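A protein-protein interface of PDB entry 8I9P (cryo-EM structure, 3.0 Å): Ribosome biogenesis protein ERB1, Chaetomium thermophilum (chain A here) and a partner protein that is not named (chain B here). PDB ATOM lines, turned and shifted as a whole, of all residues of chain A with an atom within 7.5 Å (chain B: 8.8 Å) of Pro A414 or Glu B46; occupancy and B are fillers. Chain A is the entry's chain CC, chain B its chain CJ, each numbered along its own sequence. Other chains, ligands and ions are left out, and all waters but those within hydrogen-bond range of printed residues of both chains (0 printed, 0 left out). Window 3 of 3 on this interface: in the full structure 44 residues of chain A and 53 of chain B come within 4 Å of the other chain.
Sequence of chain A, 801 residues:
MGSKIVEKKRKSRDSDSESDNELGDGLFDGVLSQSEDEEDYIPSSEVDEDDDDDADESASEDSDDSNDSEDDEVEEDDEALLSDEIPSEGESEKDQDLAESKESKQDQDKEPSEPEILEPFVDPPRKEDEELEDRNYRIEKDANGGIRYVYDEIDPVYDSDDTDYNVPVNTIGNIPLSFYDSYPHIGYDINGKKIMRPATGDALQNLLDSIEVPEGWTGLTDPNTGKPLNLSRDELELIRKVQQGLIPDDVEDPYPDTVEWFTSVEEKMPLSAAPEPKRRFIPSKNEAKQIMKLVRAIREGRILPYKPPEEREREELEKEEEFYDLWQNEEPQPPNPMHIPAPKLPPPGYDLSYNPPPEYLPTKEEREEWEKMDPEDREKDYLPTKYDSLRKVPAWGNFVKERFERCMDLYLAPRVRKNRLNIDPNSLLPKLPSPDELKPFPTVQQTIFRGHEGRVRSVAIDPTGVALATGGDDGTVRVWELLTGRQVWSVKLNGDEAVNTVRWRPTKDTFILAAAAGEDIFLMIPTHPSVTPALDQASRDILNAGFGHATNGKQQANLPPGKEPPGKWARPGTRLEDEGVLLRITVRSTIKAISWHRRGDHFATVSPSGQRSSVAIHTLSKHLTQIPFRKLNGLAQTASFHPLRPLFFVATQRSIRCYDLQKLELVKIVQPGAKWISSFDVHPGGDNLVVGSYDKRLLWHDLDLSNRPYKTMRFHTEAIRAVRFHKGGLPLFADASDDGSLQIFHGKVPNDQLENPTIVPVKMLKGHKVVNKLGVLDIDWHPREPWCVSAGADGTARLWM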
ATOM      1  N   MET A 408     -16.921 -36.001  21.741  1.00  0.00           N
ATOM      2  CA  MET A 408     -16.539 -34.622  21.454  1.00  0.00           C
ATOM      3  C   MET A 408     -17.133 -33.676  22.481  1.00  0.00           C
ATOM      4  O   MET A 408     -16.604 -32.577  22.658  1.00  0.00           O
ATOM      5  CB  MET A 408     -16.835 -34.149  20.015  1.00  0.00           C
ATOM      6  CG  MET A 408     -18.227 -34.141  19.398  1.00  0.00           C
ATOM      7  SD  MET A 408     -18.970 -35.720  19.026  1.00  0.00           S
ATOM      8  CE  MET A 408     -20.454 -35.177  18.186  1.00  0.00           C
ATOM      9  N   ASP A 409     -18.159 -34.123  23.227  1.00  0.00           N
ATOM     10  CA  ASP A 409     -18.541 -33.426  24.452  1.00  0.00           C
ATOM     11  C   ASP A 409     -17.323 -33.154  25.320  1.00  0.00           C
ATOM     12  O   ASP A 409     -16.895 -31.993  25.431  1.00  0.00           O
ATOM     13  CB  ASP A 409     -19.577 -34.234  25.233  1.00  0.00           C
ATOM     14  CG  ASP A 409     -20.999 -33.907  24.831  1.00  0.00           C
ATOM     15  OD1 ASP A 409     -21.192 -33.032  23.963  1.00  0.00           O
ATOM     16  OD2 ASP A 409     -21.927 -34.514  25.404  1.00  0.00           O
ATOM     17  N   LEU A 410     -16.624 -34.219  25.751  1.00  0.00           N
ATOM     18  CA  LEU A 410     -15.521 -34.034  26.695  1.00  0.00           C
ATOM     19  C   LEU A 410     -14.345 -33.296  26.070  1.00  0.00           C
ATOM     20  O   LEU A 410     -13.341 -33.045  26.746  1.00  0.00           O
ATOM     21  CB  LEU A 410     -15.019 -35.364  27.274  1.00  0.00           C
ATOM     22  CG  LEU A 410     -15.792 -36.464  28.011  1.00  0.00           C
ATOM     23  CD1 LEU A 410     -16.290 -37.565  27.099  1.00  0.00           C
ATOM     24  CD2 LEU A 410     -14.913 -37.042  29.117  1.00  0.00           C
ATOM     25  N   TYR A 411     -14.430 -32.942  24.785  1.00  0.00           N
ATOM     26  CA  TYR A 411     -13.319 -32.230  24.185  1.00  0.00           C
ATOM     27  C   TYR A 411     -13.774 -31.087  23.291  1.00  0.00           C
ATOM     28  O   TYR A 411     -12.931 -30.417  22.686  1.00  0.00           O
ATOM     29  CB  TYR A 411     -12.438 -33.218  23.423  1.00  0.00           C
ATOM     30  CG  TYR A 411     -11.542 -34.019  24.351  1.00  0.00           C
ATOM     31  CD1 TYR A 411     -10.296 -33.548  24.744  1.00  0.00           C
ATOM     32  CD2 TYR A 411     -11.940 -35.273  24.808  1.00  0.00           C
ATOM     33  CE1 TYR A 411      -9.485 -34.300  25.584  1.00  0.00           C
ATOM     34  CE2 TYR A 411     -11.138 -36.025  25.646  1.00  0.00           C
ATOM     35  CZ  TYR A 411      -9.911 -35.533  26.032  1.00  0.00           C
ATOM     36  OH  TYR A 411      -9.107 -36.279  26.865  1.00  0.00           O
ATOM     37  N   LEU A 412     -15.086 -30.840  23.186  1.00  0.00           N
ATOM     38  CA  LEU A 412     -15.525 -29.640  22.472  1.00  0.00           C
ATOM     39  C   LEU A 412     -16.685 -28.930  23.139  1.00  0.00           C
ATOM     40  O   LEU A 412     -17.000 -27.807  22.735  1.00  0.00           O
ATOM     41  CB  LEU A 412     -15.903 -29.969  21.018  1.00  0.00           C
ATOM     42  CG  LEU A 412     -14.798 -29.788  19.979  1.00  0.00           C
ATOM     43  CD1 LEU A 412     -15.365 -29.963  18.583  1.00  0.00           C
ATOM     44  CD2 LEU A 412     -14.140 -28.422  20.128  1.00  0.00           C
ATOM     45  N   ALA A 413     -17.361 -29.550  24.108  1.00  0.00           N
ATOM     46  CA  ALA A 413     -18.241 -28.788  24.978  1.00  0.00           C
ATOM     47  C   ALA A 413     -17.445 -28.330  26.185  1.00  0.00           C
ATOM     48  O   ALA A 413     -17.058 -29.164  27.016  1.00  0.00           O
ATOM     49  CB  ALA A 413     -19.434 -29.627  25.429  1.00  0.00           C
ATOM     50  N   PRO A 414     -17.175 -27.034  26.300  1.00  0.00           N
ATOM     51  CA  PRO A 414     -16.326 -26.539  27.388  1.00  0.00           C
ATOM     52  C   PRO A 414     -16.972 -26.712  28.754  1.00  0.00           C
ATOM     53  O   PRO A 414     -18.198 -26.716  28.900  1.00  0.00           O
ATOM     54  CB  PRO A 414     -16.140 -25.057  27.039  1.00  0.00           C
ATOM     55  CG  PRO A 414     -17.265 -24.742  26.131  1.00  0.00           C
ATOM     56  CD  PRO A 414     -17.541 -25.973  25.354  1.00  0.00           C
ATOM     57  N   ARG A 415     -16.117 -26.869  29.759  1.00  0.00           N
ATOM     58  CA  ARG A 415     -16.525 -27.180  31.122  1.00  0.00           C
ATOM     59  C   ARG A 415     -16.522 -25.906  31.953  1.00  0.00           C
ATOM     60  O   ARG A 415     -15.507 -25.204  32.015  1.00  0.00           O
ATOM     61  CB  ARG A 415     -15.590 -28.226  31.732  1.00  0.00           C
ATOM     62  CG  ARG A 415     -15.282 -29.364  30.770  1.00  0.00           C
ATOM     63  CD  ARG A 415     -14.212 -30.309  31.284  1.00  0.00           C
ATOM     64  NE  ARG A 415     -13.708 -31.157  30.210  1.00  0.00           N
ATOM     65  CZ  ARG A 415     -12.670 -31.973  30.323  1.00  0.00           C
ATOM     66  NH1 ARG A 415     -11.998 -32.082  31.457  1.00  0.00           N
ATOM     67  NH2 ARG A 415     -12.295 -32.697  29.272  1.00  0.00           N
ATOM     68  N   VAL A 416     -17.652 -25.614  32.592  1.00  0.00           N
ATOM     69  CA  VAL A 416     -17.814 -24.431  33.427  1.00  0.00           C
ATOM     70  C   VAL A 416     -17.960 -24.889  34.870  1.00  0.00           C
ATOM     71  O   VAL A 416     -18.822 -25.719  35.178  1.00  0.00           O
ATOM     72  CB  VAL A 416     -19.028 -23.589  32.993  1.00  0.00           C
ATOM     73  CG1 VAL A 416     -19.164 -22.352  33.870  1.00  0.00           C
ATOM     74  CG2 VAL A 416     -18.913 -23.206  31.524  1.00  0.00           C
ATOM     75  N   ARG A 417     -17.110 -24.361  35.744  1.00  0.00           N
ATOM     76  CA  ARG A 417     -17.155 -24.713  37.158  1.00  0.00           C
ATOM     77  C   ARG A 417     -18.350 -24.061  37.845  1.00  0.00           C
ATOM     78  O   ARG A 417     -18.561 -22.854  37.728  1.00  0.00           O
ATOM     79  CB  ARG A 417     -15.858 -24.300  37.853  1.00  0.00           C
ATOM     80  CG  ARG A 417     -15.813 -24.639  39.333  1.00  0.00           C
ATOM     81  CD  ARG A 417     -14.503 -24.187  39.950  1.00  0.00           C
ATOM     82  NE  ARG A 417     -13.367 -24.938  39.427  1.00  0.00           N
ATOM     83  CZ  ARG A 417     -12.965 -26.110  39.899  1.00  0.00           C
ATOM     84  NH1 ARG A 417     -13.589 -26.700  40.905  1.00  0.00           N
ATOM     85  NH2 ARG A 417     -11.911 -26.704  39.347  1.00  0.00           N
ATOM     86  N   ASN B  15      -5.506 -12.655  27.479  1.00  0.00           N
ATOM     87  CA  ASN B  15      -5.853 -13.827  28.274  1.00  0.00           C
ATOM     88  C   ASN B  15      -6.407 -14.953  27.413  1.00  0.00           C
ATOM     89  O   ASN B  15      -6.127 -16.129  27.671  1.00  0.00           O
ATOM     90  CB  ASN B  15      -6.860 -13.434  29.356  1.00  0.00           C
ATOM     91  CG  ASN B  15      -7.047 -14.514  30.397  1.00  0.00           C
ATOM     92  OD1 ASN B  15      -6.144 -15.312  30.644  1.00  0.00           O
ATOM     93  ND2 ASN B  15      -8.213 -14.537  31.028  1.00  0.00           N
ATOM     94  N   TYR B  16      -7.188 -14.616  26.392  1.00  0.00           N
ATOM     95  CA  TYR B  16      -7.782 -15.597  25.500  1.00  0.00           C
ATOM     96  C   TYR B  16      -7.380 -15.306  24.062  1.00  0.00           C
ATOM     97  O   TYR B  16      -7.326 -14.150  23.633  1.00  0.00           O
ATOM     98  CB  TYR B  16      -9.308 -15.607  25.631  1.00  0.00           C
ATOM     99  CG  TYR B  16      -9.789 -16.006  27.007  1.00  0.00           C
ATOM    100  CD1 TYR B  16      -9.733 -17.329  27.425  1.00  0.00           C
ATOM    101  CD2 TYR B  16     -10.277 -15.057  27.895  1.00  0.00           C
ATOM    102  CE1 TYR B  16     -10.167 -17.700  28.685  1.00  0.00           C
ATOM    103  CE2 TYR B  16     -10.713 -15.418  29.156  1.00  0.00           C
ATOM    104  CZ  TYR B  16     -10.654 -16.739  29.545  1.00  0.00           C
ATOM    105  OH  TYR B  16     -11.086 -17.100  30.801  1.00  0.00           O
ATOM    106  N   ILE B  42      -6.884 -29.902  26.004  1.00  0.00           N
ATOM    107  CA  ILE B  42      -7.193 -28.479  26.051  1.00  0.00           C
ATOM    108  C   ILE B  42      -8.637 -28.263  25.622  1.00  0.00           C
ATOM    109  O   ILE B  42      -9.058 -28.708  24.546  1.00  0.00           O
ATOM    110  CB  ILE B  42      -6.220 -27.690  25.164  1.00  0.00           C
ATOM    111  CG1 ILE B  42      -4.778 -28.115  25.454  1.00  0.00           C
ATOM    112  CG2 ILE B  42      -6.400 -26.198  25.378  1.00  0.00           C
ATOM    113  CD1 ILE B  42      -4.284 -27.710  26.827  1.00  0.00           C
ATOM    114  N   TYR B  43      -9.403 -27.574  26.462  1.00  0.00           N
ATOM    115  CA  TYR B  43     -10.807 -27.298  26.206  1.00  0.00           C
ATOM    116  C   TYR B  43     -11.026 -25.798  26.060  1.00  0.00           C
ATOM    117  O   TYR B  43     -10.362 -25.002  26.733  1.00  0.00           O
ATOM    118  CB  TYR B  43     -11.698 -27.873  27.323  1.00  0.00           C
ATOM    119  CG  TYR B  43     -11.685 -27.121  28.636  1.00  0.00           C
ATOM    120  CD1 TYR B  43     -10.522 -27.005  29.389  1.00  0.00           C
ATOM    121  CD2 TYR B  43     -12.846 -26.545  29.131  1.00  0.00           C
ATOM    122  CE1 TYR B  43     -10.514 -26.326  30.590  1.00  0.00           C
ATOM    123  CE2 TYR B  43     -12.849 -25.865  30.332  1.00  0.00           C
ATOM    124  CZ  TYR B  43     -11.679 -25.757  31.057  1.00  0.00           C
ATOM    125  OH  TYR B  43     -11.673 -25.078  32.254  1.00  0.00           O
ATOM    126  N   PRO B  44     -11.945 -25.383  25.174  1.00  0.00           N
ATOM    127  CA  PRO B  44     -11.969 -23.975  24.734  1.00  0.00           C
ATOM    128  C   PRO B  44     -12.452 -22.971  25.772  1.00  0.00           C
ATOM    129  O   PRO B  44     -12.212 -21.771  25.577  1.00  0.00           O
ATOM    130  CB  PRO B  44     -12.919 -24.000  23.527  1.00  0.00           C
ATOM    131  CG  PRO B  44     -13.771 -25.198  23.741  1.00  0.00           C
ATOM    132  CD  PRO B  44     -12.870 -26.212  24.379  1.00  0.00           C
ATOM    133  N   ARG B  45     -13.144 -23.409  26.831  1.00  0.00           N
ATOM    134  CA  ARG B  45     -13.662 -22.568  27.916  1.00  0.00           C
ATOM    135  C   ARG B  45     -14.609 -21.475  27.417  1.00  0.00           C
ATOM    136  O   ARG B  45     -15.035 -21.482  26.256  1.00  0.00           O
ATOM    137  CB  ARG B  45     -12.519 -21.922  28.712  1.00  0.00           C
ATOM    138  CG  ARG B  45     -11.381 -22.851  29.102  1.00  0.00           C
ATOM    139  CD  ARG B  45     -10.235 -22.053  29.705  1.00  0.00           C
ATOM    140  NE  ARG B  45      -9.028 -22.855  29.863  1.00  0.00           N
ATOM    141  CZ  ARG B  45      -8.683 -23.480  30.978  1.00  0.00           C
ATOM    142  NH1 ARG B  45      -9.435 -23.418  32.064  1.00  0.00           N
ATOM    143  NH2 ARG B  45      -7.567 -24.202  30.998  1.00  0.00           N
ATOM    144  N   GLU B  46     -14.967 -20.541  28.311  1.00  0.00           N
ATOM    145  CA  GLU B  46     -15.620 -19.283  27.952  1.00  0.00           C
ATOM    146  C   GLU B  46     -14.843 -18.134  28.579  1.00  0.00           C
ATOM    147  O   GLU B  46     -14.399 -18.238  29.729  1.00  0.00           O
ATOM    148  CB  GLU B  46     -17.080 -19.170  28.424  1.00  0.00           C
ATOM    149  CG  GLU B  46     -18.129 -20.063  27.797  1.00  0.00           C
ATOM    150  CD  GLU B  46     -17.981 -21.526  28.134  1.00  0.00           C
ATOM    151  OE1 GLU B  46     -17.184 -21.877  29.029  1.00  0.00           O
ATOM    152  OE2 GLU B  46     -18.680 -22.335  27.499  1.00  0.00           O
ATOM    153  N   PRO B  47     -14.598 -17.060  27.836  1.00  0.00           N
ATOM    154  CA  PRO B  47     -14.245 -15.788  28.471  1.00  0.00           C
ATOM    155  C   PRO B  47     -15.445 -15.192  29.183  1.00  0.00           C
ATOM    156  O   PRO B  47     -16.598 -15.513  28.887  1.00  0.00           O
ATOM    157  CB  PRO B  47     -13.810 -14.901  27.299  1.00  0.00           C
ATOM    158  CG  PRO B  47     -13.607 -15.830  26.146  1.00  0.00           C
ATOM    159  CD  PRO B  47     -14.538 -16.981  26.368  1.00  0.00           C
ATOM    160  N   ARG B  48     -15.155 -14.303  30.136  1.00  0.00           N
ATOM    161  CA  ARG B  48     -16.223 -13.531  30.762  1.00  0.00           C
ATOM    162  C   ARG B  48     -16.889 -12.604  29.752  1.00  0.00           C
ATOM    163  O   ARG B  48     -18.112 -12.418  29.779  1.00  0.00           O
ATOM    164  CB  ARG B  48     -15.676 -12.737  31.947  1.00  0.00           C
ATOM    165  CG  ARG B  48     -16.753 -12.099  32.808  1.00  0.00           C
ATOM    166  CD  ARG B  48     -16.304 -10.748  33.332  1.00  0.00           C
ATOM    167  NE  ARG B  48     -16.758  -9.657  32.479  1.00  0.00           N
ATOM    168  CZ  ARG B  48     -15.949  -8.804  31.865  1.00  0.00           C
ATOM    169  NH1 ARG B  48     -14.634  -8.894  31.982  1.00  0.00           N
ATOM    170  NH2 ARG B  48     -16.471  -7.840  31.113  1.00  0.00           N
ATOM    171  N   ASP B  49     -16.101 -12.022  28.852  1.00  0.00           N
ATOM    172  CA  ASP B  49     -16.619 -11.172  27.785  1.00  0.00           C
ATOM    173  C   ASP B  49     -15.903 -11.540  26.493  1.00  0.00           C
ATOM    174  O   ASP B  49     -14.706 -11.273  26.350  1.00  0.00           O
ATOM    175  CB  ASP B  49     -16.422  -9.691  28.111  1.00  0.00           C
ATOM    176  CG  ASP B  49     -17.364  -8.793  27.335  1.00  0.00           C
ATOM    177  OD1 ASP B  49     -18.291  -9.324  26.687  1.00  0.00           O
ATOM    178  OD2 ASP B  49     -17.176  -7.559  27.370  1.00  0.00           O
ATOM    179  N   ARG B  50     -16.631 -12.152  25.555  1.00  0.00           N
ATOM    180  CA  ARG B  50     -16.077 -12.403  24.228  1.00  0.00           C
ATOM    181  C   ARG B  50     -15.914 -11.116  23.431  1.00  0.00           C
ATOM    182  O   ARG B  50     -15.152 -11.089  22.458  1.00  0.00           O
ATOM    183  CB  ARG B  50     -16.962 -13.393  23.467  1.00  0.00           C
ATOM    184  CG  ARG B  50     -18.356 -12.873  23.147  1.00  0.00           C
ATOM    185  CD  ARG B  50     -19.182 -13.903  22.389  1.00  0.00           C
ATOM    186  NE  ARG B  50     -19.549 -15.037  23.229  1.00  0.00           N
ATOM    187  CZ  ARG B  50     -19.100 -16.274  23.061  1.00  0.00           C
ATOM    188  NH1 ARG B  50     -18.261 -16.578  22.084  1.00  0.00           N
ATOM    189  NH2 ARG B  50     -19.504 -17.230  23.893  1.00  0.00           N
ATOM    190  N   VAL B  53     -12.283  -9.743  24.035  1.00  0.00           N
ATOM    191  CA  VAL B  53     -11.149 -10.539  23.571  1.00  0.00           C
ATOM    192  C   VAL B  53     -10.617  -9.995  22.248  1.00  0.00           C
ATOM    193  O   VAL B  53      -9.454  -9.589  22.149  1.00  0.00           O
ATOM    194  CB  VAL B  53     -11.542 -12.023  23.457  1.00  0.00           C
ATOM    195  CG1 VAL B  53     -10.354 -12.848  22.988  1.00  0.00           C
ATOM    196  CG2 VAL B  53     -12.055 -12.538  24.790  1.00  0.00           C
ATOM    197  N   ALA B  59     -20.262 -15.460  18.347  1.00  0.00           N
ATOM    198  CA  ALA B  59     -20.536 -16.475  19.360  1.00  0.00           C
ATOM    199  C   ALA B  59     -20.240 -17.888  18.873  1.00  0.00           C
ATOM    200  O   ALA B  59     -20.007 -18.778  19.697  1.00  0.00           O
ATOM    201  CB  ALA B  59     -21.992 -16.378  19.818  1.00  0.00           C
ATOM    202  N   THR B  61     -17.582 -18.668  17.169  1.00  0.00           N
ATOM    203  CA  THR B  61     -16.142 -18.845  17.284  1.00  0.00           C
ATOM    204  C   THR B  61     -15.761 -19.308  18.687  1.00  0.00           C
ATOM    205  O   THR B  61     -16.410 -18.966  19.679  1.00  0.00           O
ATOM    206  CB  THR B  61     -15.410 -17.544  16.952  1.00  0.00           C
ATOM    207  OG1 THR B  61     -15.602 -16.600  18.014  1.00  0.00           O
ATOM    208  CG2 THR B  61     -15.934 -16.954  15.652  1.00  0.00           C
ATOM    209  N   THR B  62     -14.691 -20.093  18.759  1.00  0.00           N
ATOM    210  CA  THR B  62     -14.198 -20.649  20.012  1.00  0.00           C
ATOM    211  C   THR B  62     -12.847 -20.037  20.358  1.00  0.00           C
ATOM    212  O   THR B  62     -12.040 -19.743  19.469  1.00  0.00           O
ATOM    213  CB  THR B  62     -14.071 -22.173  19.927  1.00  0.00           C
ATOM    214  OG1 THR B  62     -13.133 -22.521  18.904  1.00  0.00           O
ATOM    215  CG2 THR B  62     -15.420 -22.803  19.608  1.00  0.00           C
ATOM    216  N   PHE B  63     -12.608 -19.850  21.651  1.00  0.00           N
ATOM    217  CA  PHE B  63     -11.386 -19.253  22.170  1.00  0.00           C
ATOM    218  C   PHE B  63     -10.540 -20.325  22.848  1.00  0.00           C
ATOM    219  O   PHE B  63     -10.909 -21.499  22.902  1.00  0.00           O
ATOM    220  CB  PHE B  63     -11.715 -18.114  23.138  1.00  0.00           C
ATOM    221  CG  PHE B  63     -12.664 -17.093  22.577  1.00  0.00           C
ATOM    222  CD1 PHE B  63     -12.193 -16.036  21.816  1.00  0.00           C
ATOM    223  CD2 PHE B  63     -14.026 -17.189  22.815  1.00  0.00           C
ATOM    224  CE1 PHE B  63     -13.065 -15.097  21.299  1.00  0.00           C
ATOM    225  CE2 PHE B  63     -14.903 -16.251  22.302  1.00  0.00           C
ATOM    226  CZ  PHE B  63     -14.420 -15.204  21.543  1.00  0.00           C
ATOM    227  N   TYR B  64      -9.388 -19.909  23.371  1.00  0.00           N
ATOM    228  CA  TYR B  64      -8.488 -20.813  24.069  1.00  0.00           C
ATOM    229  C   TYR B  64      -7.667 -20.020  25.075  1.00  0.00           C
ATOM    230  O   TYR B  64      -7.409 -18.826  24.887  1.00  0.00           O
ATOM    231  CB  TYR B  64      -7.552 -21.546  23.098  1.00  0.00           C
ATOM    232  CG  TYR B  64      -8.136 -22.805  22.500  1.00  0.00           C
ATOM    233  CD1 TYR B  64      -8.257 -23.965  23.253  1.00  0.00           C
ATOM    234  CD2 TYR B  64      -8.554 -22.838  21.175  1.00  0.00           C
ATOM    235  CE1 TYR B  64      -8.787 -25.121  22.709  1.00  0.00           C
ATOM    236  CE2 TYR B  64      -9.086 -23.987  20.621  1.00  0.00           C
ATOM    237  CZ  TYR B  64      -9.200 -25.126  21.392  1.00  0.00           C
ATOM    238  OH  TYR B  64      -9.728 -26.273  20.846  1.00  0.00           O
ATOM    239  N   TYR B  65      -7.257 -20.702  26.141  1.00  0.00           N
ATOM    240  CA  TYR B  65      -6.400 -20.100  27.153  1.00  0.00           C
ATOM    241  C   TYR B  65      -4.997 -19.866  26.605  1.00  0.00           C
ATOM    242  O   TYR B  65      -4.439 -20.714  25.905  1.00  0.00           O
ATOM    243  CB  TYR B  65      -6.340 -21.000  28.386  1.00  0.00           C
ATOM    244  CG  TYR B  65      -5.810 -20.332  29.632  1.00  0.00           C
ATOM    245  CD1 TYR B  65      -6.019 -18.979  29.866  1.00  0.00           C
ATOM    246  CD2 TYR B  65      -5.096 -21.059  30.576  1.00  0.00           C
ATOM    247  CE1 TYR B  65      -5.529 -18.371  31.008  1.00  0.00           C
ATOM    248  CE2 TYR B  65      -4.604 -20.460  31.720  1.00  0.00           C
ATOM    249  CZ  TYR B  65      -4.823 -19.116  31.930  1.00  0.00           C
ATOM    250  OH  TYR B  65      -4.335 -18.514  33.067  1.00  0.00           O
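No residue of chain B comes within 4 Å of Ala A413.
Pro A414 touches just these residues of chain B: Tyr B43, Arg B45 and Glu B46.
Of the printed residues of chain B, Arg A415 touches Tyr B43 (3.2 Å).
Of the printed residues of chain A, Tyr B43 touches Pro A414 and Arg A415.
Printed residues of chain A within 4 Å of Arg B45: Pro A414 (3.4 Å).
Glu B46 touches two residues of chain A.
The nearest residue of chain A that does not touch Glu B46 is Arg A415 (4.8 Å).
Pro A414 touches Tyr B43.
CB of Pro A414 touches N of Arg B45 (3.4 Å).
OE2 of Glu B46 touches CG of Pro A414, 3.1 Å away.
Tyr B43 touches Arg A415.
Glu B46 touches Val A416.
NH1 of Arg B45 lies within hydrogen-bond range of OH of Tyr B43 (2.8 Å).
O of Leu A410 lies within hydrogen-bond range of NH2 of Arg A415.
Of the 18 printed residues of chain B, 3 touch a printed residue of chain A.
Hydrophobic or aromatic side chains of chain B within 4 Å of the printed part of chain A: Tyr B43.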
